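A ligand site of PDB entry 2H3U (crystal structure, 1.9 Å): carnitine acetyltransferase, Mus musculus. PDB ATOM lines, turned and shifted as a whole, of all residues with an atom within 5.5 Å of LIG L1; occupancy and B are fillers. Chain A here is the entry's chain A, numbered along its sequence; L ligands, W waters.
Water W3 lies within hydrogen-bond range of the side-chain hydroxyl (OH) of Tyr 81 (2.6 Å), an oxygen (O1) of LIG L1 (2.7 Å), the side-chain carboxylate (OE1) of Glu 321 (2.9 Å) and the indole nitrogen (NE1) of Trp 76 (2.9 Å).
Water W4 lies within hydrogen-bond range of OG of Ser 528 (2.8 Å), S1 of LG2 L2 (2.9 Å) and O3 of LIG L1 (3.0 Å).
Water W2 lies within hydrogen-bond range of OH of Tyr 426 (2.8 Å) and O1 of LIG L1 (3.3 Å).
The side-chain hydroxyl (OH) of Tyr 426 is in hydrogen-bond range of an oxygen (O2) of LIG L1, at 2.6 Å.
A ring nitrogen (NE2) of His 317 lies within hydrogen-bond range of an oxygen (O3) of LIG L1, 2.8 Å away.
O2 of LIG L1 is in hydrogen-bond range of OG of Ser 428, at 2.7 Å.
OG1 of Thr 439 lies within hydrogen-bond range of O1 of LIG L1, at 2.7 Å.
A ring nitrogen (ND1) of His 317 lies within hydrogen-bond range of the side-chain hydroxyl (OH) of Tyr 81 (3.2 Å).
The backbone carbonyl oxygen (O) of Tyr 426 is in hydrogen-bond range of the backbone NH (N) of Thr 527 (2.8 Å).
N of Ser 428 sits at hydrogen-bond distance from O of Thr 527.
The guanidinium group of Arg 492 is in hydrogen-bond range of the backbone carbonyl oxygen of Thr 439 (3.0 Å).
OH of Tyr 426 lies within hydrogen-bond range of NH2 of Arg 492, 2.8 Å away.
S1 of LG2 L2 lies close to O3 of LIG L1 (2.9 Å).
Trp 76 touches LIG L1 (CZ2 to O1, 3.5 Å).
Tyr 81 touches LIG L1.
Ser 526 touches LIG L1 (OG to C7, 3.2 Å).
Thr 527 touches LIG L1.
Phe 540 touches LIG L1 (CE2 to C6, 3.6 Å).
CG1 of Val 543 touches C7 of LIG L1, 3.6 Å away.
Hydrophobic or aromatic side chains that line LIG L1: Trp 76, His 317, Tyr 426, Phe 540 and Val 543.
Ten residues have an atom within 4 Å of LIG L1: Trp 76, Tyr 81, His 317, Tyr 426, Ser 428, Thr 439, Ser 526, Thr 527, Phe 540 and Val 543.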
ATOM      1  N   TRP A  76     -23.508 -42.524  26.797  1.00  0.00           N
ATOM      2  CA  TRP A  76     -23.005 -41.181  27.086  1.00  0.00           C
ATOM      3  C   TRP A  76     -23.670 -40.559  28.300  1.00  0.00           C
ATOM      4  O   TRP A  76     -22.999 -39.955  29.134  1.00  0.00           O
ATOM      5  CB  TRP A  76     -23.206 -40.260  25.876  1.00  0.00           C
ATOM      6  CG  TRP A  76     -22.679 -38.862  26.119  1.00  0.00           C
ATOM      7  CD1 TRP A  76     -23.417 -37.705  26.247  1.00  0.00           C
ATOM      8  CD2 TRP A  76     -21.316 -38.482  26.280  1.00  0.00           C
ATOM      9  NE1 TRP A  76     -22.582 -36.644  26.479  1.00  0.00           N
ATOM     10  CE2 TRP A  76     -21.281 -37.082  26.508  1.00  0.00           C
ATOM     11  CE3 TRP A  76     -20.098 -39.189  26.268  1.00  0.00           C
ATOM     12  CZ2 TRP A  76     -20.091 -36.379  26.713  1.00  0.00           C
ATOM     13  CZ3 TRP A  76     -18.908 -38.486  26.472  1.00  0.00           C
ATOM     14  CH2 TRP A  76     -18.914 -37.098  26.691  1.00  0.00           C
ATOM     15  N   TYR A  81     -22.679 -38.222  32.890  1.00  0.00           N
ATOM     16  CA  TYR A  81     -23.423 -37.610  33.993  1.00  0.00           C
ATOM     17  C   TYR A  81     -23.972 -38.484  35.121  1.00  0.00           C
ATOM     18  O   TYR A  81     -23.613 -38.278  36.289  1.00  0.00           O
ATOM     19  CB  TYR A  81     -24.586 -36.764  33.458  1.00  0.00           C
ATOM     20  CG  TYR A  81     -24.170 -35.811  32.360  1.00  0.00           C
ATOM     21  CD1 TYR A  81     -24.463 -36.069  31.028  1.00  0.00           C
ATOM     22  CD2 TYR A  81     -23.423 -34.664  32.663  1.00  0.00           C
ATOM     23  CE1 TYR A  81     -24.017 -35.227  30.013  1.00  0.00           C
ATOM     24  CE2 TYR A  81     -22.977 -33.822  31.658  1.00  0.00           C
ATOM     25  CZ  TYR A  81     -23.269 -34.100  30.338  1.00  0.00           C
ATOM     26  OH  TYR A  81     -22.787 -33.258  29.364  1.00  0.00           O
ATOM     27  N   PRO A  94     -23.552 -26.126  34.266  1.00  0.00           N
ATOM     28  CA  PRO A  94     -23.031 -24.849  33.788  1.00  0.00           C
ATOM     29  C   PRO A  94     -23.804 -23.672  34.356  1.00  0.00           C
ATOM     30  O   PRO A  94     -25.014 -23.770  34.618  1.00  0.00           O
ATOM     31  CB  PRO A  94     -23.204 -24.947  32.268  1.00  0.00           C
ATOM     32  CG  PRO A  94     -23.250 -26.415  31.997  1.00  0.00           C
ATOM     33  CD  PRO A  94     -24.067 -26.939  33.154  1.00  0.00           C
ATOM     34  N   TYR A 315     -28.077 -24.718  35.079  1.00  0.00           N
ATOM     35  CA  TYR A 315     -28.909 -25.843  34.673  1.00  0.00           C
ATOM     36  C   TYR A 315     -28.196 -27.175  34.845  1.00  0.00           C
ATOM     37  O   TYR A 315     -26.975 -27.250  34.723  1.00  0.00           O
ATOM     38  CB  TYR A 315     -29.379 -25.662  33.220  1.00  0.00           C
ATOM     39  CG  TYR A 315     -28.343 -25.968  32.166  1.00  0.00           C
ATOM     40  CD1 TYR A 315     -28.197 -27.265  31.666  1.00  0.00           C
ATOM     41  CD2 TYR A 315     -27.533 -24.974  31.641  1.00  0.00           C
ATOM     42  CE1 TYR A 315     -27.268 -27.555  30.680  1.00  0.00           C
ATOM     43  CE2 TYR A 315     -26.587 -25.255  30.643  1.00  0.00           C
ATOM     44  CZ  TYR A 315     -26.472 -26.554  30.174  1.00  0.00           C
ATOM     45  OH  TYR A 315     -25.562 -26.833  29.176  1.00  0.00           O
ATOM     46  N   HIS A 317     -26.875 -30.433  33.717  1.00  0.00           N
ATOM     47  CA  HIS A 317     -26.381 -30.917  32.426  1.00  0.00           C
ATOM     48  C   HIS A 317     -26.902 -32.214  31.830  1.00  0.00           C
ATOM     49  O   HIS A 317     -26.845 -32.391  30.612  1.00  0.00           O
ATOM     50  CB  HIS A 317     -24.848 -30.985  32.467  1.00  0.00           C
ATOM     51  CG  HIS A 317     -24.190 -30.513  31.213  1.00  0.00           C
ATOM     52  ND1 HIS A 317     -24.731 -30.726  29.964  1.00  0.00           N
ATOM     53  CD2 HIS A 317     -23.024 -29.846  31.019  1.00  0.00           C
ATOM     54  CE1 HIS A 317     -23.919 -30.211  29.049  1.00  0.00           C
ATOM     55  NE2 HIS A 317     -22.882 -29.672  29.653  1.00  0.00           N
ATOM     56  N   GLU A 321     -27.565 -29.585  26.223  1.00  0.00           N
ATOM     57  CA  GLU A 321     -26.373 -28.781  26.003  1.00  0.00           C
ATOM     58  C   GLU A 321     -26.792 -27.320  26.040  1.00  0.00           C
ATOM     59  O   GLU A 321     -27.959 -27.005  26.197  1.00  0.00           O
ATOM     60  CB  GLU A 321     -25.747 -29.075  24.632  1.00  0.00           C
ATOM     61  CG  GLU A 321     -24.608 -30.073  24.662  1.00  0.00           C
ATOM     62  CD  GLU A 321     -25.069 -31.420  25.138  1.00  0.00           C
ATOM     63  OE1 GLU A 321     -24.883 -31.733  26.321  1.00  0.00           O
ATOM     64  OE2 GLU A 321     -25.636 -32.173  24.311  1.00  0.00           O
ATOM     65  N   TYR A 426     -10.208 -30.117  24.367  1.00  0.00           N
ATOM     66  CA  TYR A 426     -11.569 -30.534  24.079  1.00  0.00           C
ATOM     67  C   TYR A 426     -12.454 -29.342  23.719  1.00  0.00           C
ATOM     68  O   TYR A 426     -12.417 -28.303  24.390  1.00  0.00           O
ATOM     69  CB  TYR A 426     -12.149 -31.192  25.334  1.00  0.00           C
ATOM     70  CG  TYR A 426     -13.574 -31.702  25.237  1.00  0.00           C
ATOM     71  CD1 TYR A 426     -13.821 -33.067  25.234  1.00  0.00           C
ATOM     72  CD2 TYR A 426     -14.659 -30.829  25.162  1.00  0.00           C
ATOM     73  CE1 TYR A 426     -15.127 -33.568  25.148  1.00  0.00           C
ATOM     74  CE2 TYR A 426     -15.974 -31.311  25.083  1.00  0.00           C
ATOM     75  CZ  TYR A 426     -16.194 -32.685  25.071  1.00  0.00           C
ATOM     76  OH  TYR A 426     -17.477 -33.164  24.962  1.00  0.00           O
ATOM     77  N   SER A 428     -16.580 -28.770  22.534  1.00  0.00           N
ATOM     78  CA  SER A 428     -17.876 -29.365  22.277  1.00  0.00           C
ATOM     79  C   SER A 428     -18.304 -29.241  20.821  1.00  0.00           C
ATOM     80  O   SER A 428     -18.209 -28.153  20.239  1.00  0.00           O
ATOM     81  CB  SER A 428     -18.952 -28.712  23.141  1.00  0.00           C
ATOM     82  OG  SER A 428     -18.650 -28.822  24.524  1.00  0.00           O
ATOM     83  N   ALA A 429     -18.765 -30.352  20.255  1.00  0.00           N
ATOM     84  CA  ALA A 429     -19.255 -30.378  18.885  1.00  0.00           C
ATOM     85  C   ALA A 429     -20.670 -30.954  18.967  1.00  0.00           C
ATOM     86  O   ALA A 429     -20.878 -31.997  19.583  1.00  0.00           O
ATOM     87  CB  ALA A 429     -18.381 -31.248  18.003  1.00  0.00           C
ATOM     88  N   THR A 439     -23.337 -34.750  21.707  1.00  0.00           N
ATOM     89  CA  THR A 439     -22.069 -34.166  21.301  1.00  0.00           C
ATOM     90  C   THR A 439     -20.943 -35.134  20.954  1.00  0.00           C
ATOM     91  O   THR A 439     -21.027 -36.333  21.217  1.00  0.00           O
ATOM     92  CB  THR A 439     -21.513 -33.261  22.413  1.00  0.00           C
ATOM     93  OG1 THR A 439     -21.133 -34.082  23.533  1.00  0.00           O
ATOM     94  CG2 THR A 439     -22.565 -32.250  22.877  1.00  0.00           C
ATOM     95  N   ASP A 440     -19.878 -34.592  20.361  1.00  0.00           N
ATOM     96  CA  ASP A 440     -18.679 -35.352  20.082  1.00  0.00           C
ATOM     97  C   ASP A 440     -17.536 -34.388  20.388  1.00  0.00           C
ATOM     98  O   ASP A 440     -17.779 -33.221  20.720  1.00  0.00           O
ATOM     99  CB  ASP A 440     -18.583 -35.832  18.637  1.00  0.00           C
ATOM    100  CG  ASP A 440     -17.768 -37.109  18.493  1.00  0.00           C
ATOM    101  OD1 ASP A 440     -16.850 -37.333  19.330  1.00  0.00           O
ATOM    102  OD2 ASP A 440     -18.011 -37.902  17.552  1.00  0.00           O
ATOM    103  N   ARG A 492     -16.032 -40.235  20.623  1.00  0.00           N
ATOM    104  CA  ARG A 492     -17.177 -41.020  21.082  1.00  0.00           C
ATOM    105  C   ARG A 492     -17.093 -42.436  20.544  1.00  0.00           C
ATOM    106  O   ARG A 492     -17.534 -43.385  21.188  1.00  0.00           O
ATOM    107  CB  ARG A 492     -18.489 -40.372  20.627  1.00  0.00           C
ATOM    108  CG  ARG A 492     -18.741 -38.997  21.218  1.00  0.00           C
ATOM    109  CD  ARG A 492     -18.958 -39.000  22.735  1.00  0.00           C
ATOM    110  NE  ARG A 492     -19.178 -37.614  23.174  1.00  0.00           N
ATOM    111  CZ  ARG A 492     -18.206 -36.726  23.336  1.00  0.00           C
ATOM    112  NH1 ARG A 492     -16.939 -37.083  23.135  1.00  0.00           N
ATOM    113  NH2 ARG A 492     -18.497 -35.473  23.649  1.00  0.00           N
ATOM    114  N   SER A 526     -10.644 -27.609  28.514  1.00  0.00           N
ATOM    115  CA  SER A 526     -11.979 -28.117  28.206  1.00  0.00           C
ATOM    116  C   SER A 526     -12.737 -26.871  27.801  1.00  0.00           C
ATOM    117  O   SER A 526     -12.817 -25.919  28.580  1.00  0.00           O
ATOM    118  CB  SER A 526     -12.627 -28.756  29.448  1.00  0.00           C
ATOM    119  OG  SER A 526     -13.928 -29.222  29.146  1.00  0.00           O
ATOM    120  N   THR A 527     -13.291 -26.868  26.598  1.00  0.00           N
ATOM    121  CA  THR A 527     -13.966 -25.680  26.089  1.00  0.00           C
ATOM    122  C   THR A 527     -15.233 -25.920  25.290  1.00  0.00           C
ATOM    123  O   THR A 527     -15.547 -27.035  24.877  1.00  0.00           O
ATOM    124  CB  THR A 527     -13.034 -24.904  25.167  1.00  0.00           C
ATOM    125  OG1 THR A 527     -13.009 -25.531  23.888  1.00  0.00           O
ATOM    126  CG2 THR A 527     -11.613 -24.904  25.742  1.00  0.00           C
ATOM    127  N   SER A 528     -15.954 -24.831  25.043  1.00  0.00           N
ATOM    128  CA  SER A 528     -17.175 -24.884  24.244  1.00  0.00           C
ATOM    129  C   SER A 528     -17.585 -23.480  23.854  1.00  0.00           C
ATOM    130  O   SER A 528     -17.246 -22.492  24.523  1.00  0.00           O
ATOM    131  CB  SER A 528     -18.326 -25.544  25.021  1.00  0.00           C
ATOM    132  OG  SER A 528     -18.820 -24.670  26.017  1.00  0.00           O
ATOM    133  N   PHE A 540     -18.169 -22.987  33.443  1.00  0.00           N
ATOM    134  CA  PHE A 540     -18.172 -24.275  34.139  1.00  0.00           C
ATOM    135  C   PHE A 540     -16.778 -24.500  34.678  1.00  0.00           C
ATOM    136  O   PHE A 540     -15.834 -23.871  34.215  1.00  0.00           O
ATOM    137  CB  PHE A 540     -18.559 -25.392  33.162  1.00  0.00           C
ATOM    138  CG  PHE A 540     -17.793 -25.371  31.868  1.00  0.00           C
ATOM    139  CD1 PHE A 540     -16.506 -25.899  31.786  1.00  0.00           C
ATOM    140  CD2 PHE A 540     -18.348 -24.798  30.724  1.00  0.00           C
ATOM    141  CE1 PHE A 540     -15.778 -25.842  30.579  1.00  0.00           C
ATOM    142  CE2 PHE A 540     -17.642 -24.743  29.516  1.00  0.00           C
ATOM    143  CZ  PHE A 540     -16.355 -25.268  29.454  1.00  0.00           C
ATOM    144  N   VAL A 543     -12.351 -29.780  33.899  1.00  0.00           N
ATOM    145  CA  VAL A 543     -12.678 -31.198  34.013  1.00  0.00           C
ATOM    146  C   VAL A 543     -11.544 -32.004  34.644  1.00  0.00           C
ATOM    147  O   VAL A 543     -11.692 -33.189  34.934  1.00  0.00           O
ATOM    148  CB  VAL A 543     -13.047 -31.801  32.637  1.00  0.00           C
ATOM    149  CG1 VAL A 543     -14.198 -31.027  32.009  1.00  0.00           C
ATOM    150  CG2 VAL A 543     -11.831 -31.777  31.709  1.00  0.00           C
HETATM  151  C1  LIG L   1     -20.230 -31.779  26.054  1.00  0.00           C
HETATM  152  O1  LIG L   1     -20.631 -32.972  25.991  1.00  0.00           O
HETATM  153  O2  LIG L   1     -19.321 -31.340  25.319  1.00  0.00           O
HETATM  154  C2  LIG L   1     -20.879 -30.829  27.050  1.00  0.00           C
HETATM  155  C3  LIG L   1     -19.916 -29.744  27.573  1.00  0.00           C
HETATM  156  O3  LIG L   1     -20.687 -28.730  28.219  1.00  0.00           O
HETATM  157  C4  LIG L   1     -18.970 -30.380  28.587  1.00  0.00           C
HETATM  158  N1  LIG L   1     -17.842 -29.489  28.931  1.00  0.00           N
HETATM  159  C5  LIG L   1     -17.113 -29.100  27.717  1.00  0.00           C
HETATM  160  C6  LIG L   1     -18.334 -28.293  29.610  1.00  0.00           C
HETATM  161  C7  LIG L   1     -16.936 -30.207  29.823  1.00  0.00           C
HETATM  162  N1  LG2 L   2     -15.391 -16.628   6.015  1.00  0.00           N
HETATM  163  C1  LG2 L   2     -16.348 -15.778   6.416  1.00  0.00           C
HETATM  164  N2  LG2 L   2     -17.259 -16.153   7.325  1.00  0.00           N
HETATM  165  C2  LG2 L   2     -17.218 -17.388   7.874  1.00  0.00           C
HETATM  166  C3  LG2 L   2     -16.233 -18.289   7.488  1.00  0.00           C
HETATM  167  C4  LG2 L   2     -15.301 -17.873   6.535  1.00  0.00           C
HETATM  168  N3  LG2 L   2     -14.345 -18.701   6.131  1.00  0.00           N
HETATM  169  N4  LG2 L   2     -16.417 -19.415   8.164  1.00  0.00           N
HETATM  170  C5  LG2 L   2     -17.483 -19.245   8.961  1.00  0.00           C
HETATM  171  N5  LG2 L   2     -17.977 -18.001   8.780  1.00  0.00           N
HETATM  172  C6  LG2 L   2     -19.163 -17.394   9.467  1.00  0.00           C
HETATM  173  C7  LG2 L   2     -20.340 -18.338   9.602  1.00  0.00           C
HETATM  174  O1  LG2 L   2     -21.120 -18.276   8.391  1.00  0.00           O
HETATM  175  C8  LG2 L   2     -21.121 -17.720  10.734  1.00  0.00           C
HETATM  176  O2  LG2 L   2     -21.842 -16.589  10.251  1.00  0.00           O
HETATM  177  P1  LG2 L   2     -22.900 -15.836  11.196  1.00  0.00           P
HETATM  178  O3  LG2 L   2     -23.711 -14.885  10.179  1.00  0.00           O
HETATM  179  O4  LG2 L   2     -23.812 -16.847  11.772  1.00  0.00           O
HETATM  180  O5  LG2 L   2     -22.132 -14.963  12.112  1.00  0.00           O
HETATM  181  C9  LG2 L   2     -20.028 -17.248  11.698  1.00  0.00           C
HETATM  182  O6  LG2 L   2     -18.839 -16.998  10.855  1.00  0.00           O
HETATM  183  C10 LG2 L   2     -19.655 -18.334  12.736  1.00  0.00           C
HETATM  184  O7  LG2 L   2     -19.146 -19.515  12.106  1.00  0.00           O
HETATM  185  P2  LG2 L   2     -18.006 -20.384  12.855  1.00  0.00           P
HETATM  186  O8  LG2 L   2     -17.187 -19.447  13.675  1.00  0.00           O
HETATM  187  O9  LG2 L   2     -17.320 -21.255  11.870  1.00  0.00           O
HETATM  188  O10 LG2 L   2     -18.849 -21.291  13.904  1.00  0.00           O
HETATM  189  P3  LG2 L   2     -20.039 -22.286  13.450  1.00  0.00           P
HETATM  190  O11 LG2 L   2     -19.651 -23.049  12.239  1.00  0.00           O
HETATM  191  O12 LG2 L   2     -21.321 -21.528  13.416  1.00  0.00           O
HETATM  192  O13 LG2 L   2     -20.104 -23.306  14.678  1.00  0.00           O
HETATM  193  C11 LG2 L   2     -19.401 -25.101  16.160  1.00  0.00           C
HETATM  194  C12 LG2 L   2     -19.048 -24.255  14.933  1.00  0.00           C
HETATM  195  C13 LG2 L   2     -19.464 -24.179  17.396  1.00  0.00           C
HETATM  196  C14 LG2 L   2     -18.310 -26.161  16.377  1.00  0.00           C
HETATM  197  C15 LG2 L   2     -20.784 -25.767  15.910  1.00  0.00           C
HETATM  198  O14 LG2 L   2     -20.697 -26.639  14.789  1.00  0.00           O
HETATM  199  C16 LG2 L   2     -21.257 -26.540  17.138  1.00  0.00           C
HETATM  200  O15 LG2 L   2     -20.988 -27.729  17.291  1.00  0.00           O
HETATM  201  N6  LG2 L   2     -21.964 -25.809  18.007  1.00  0.00           N
HETATM  202  C17 LG2 L   2     -22.512 -26.360  19.240  1.00  0.00           C
HETATM  203  C18 LG2 L   2     -21.438 -26.363  20.356  1.00  0.00           C
HETATM  204  C19 LG2 L   2     -22.082 -26.773  21.674  1.00  0.00           C
HETATM  205  O16 LG2 L   2     -22.695 -27.835  21.765  1.00  0.00           O
HETATM  206  N7  LG2 L   2     -21.927 -25.897  22.665  1.00  0.00           N
HETATM  207  C20 LG2 L   2     -22.512 -26.097  24.030  1.00  0.00           C
HETATM  208  C21 LG2 L   2     -21.856 -27.271  24.749  1.00  0.00           C
HETATM  209  S1  LG2 L   2     -22.630 -27.580  26.376  1.00  0.00           S
HETATM  210  O   HOH W   1     -19.793 -28.966  32.660  1.00  0.00           O
HETATM  211  O   HOH W   2     -17.904 -33.783  27.613  1.00  0.00           O
HETATM  212  O   HOH W   3     -23.032 -33.841  26.861  1.00  0.00           O
HETATM  213  O   HOH W   4     -20.817 -25.749  27.608  1.00  0.00           O
HETATM  214  O   HOH W   5     -19.867 -33.450  29.551  1.00  0.00           O
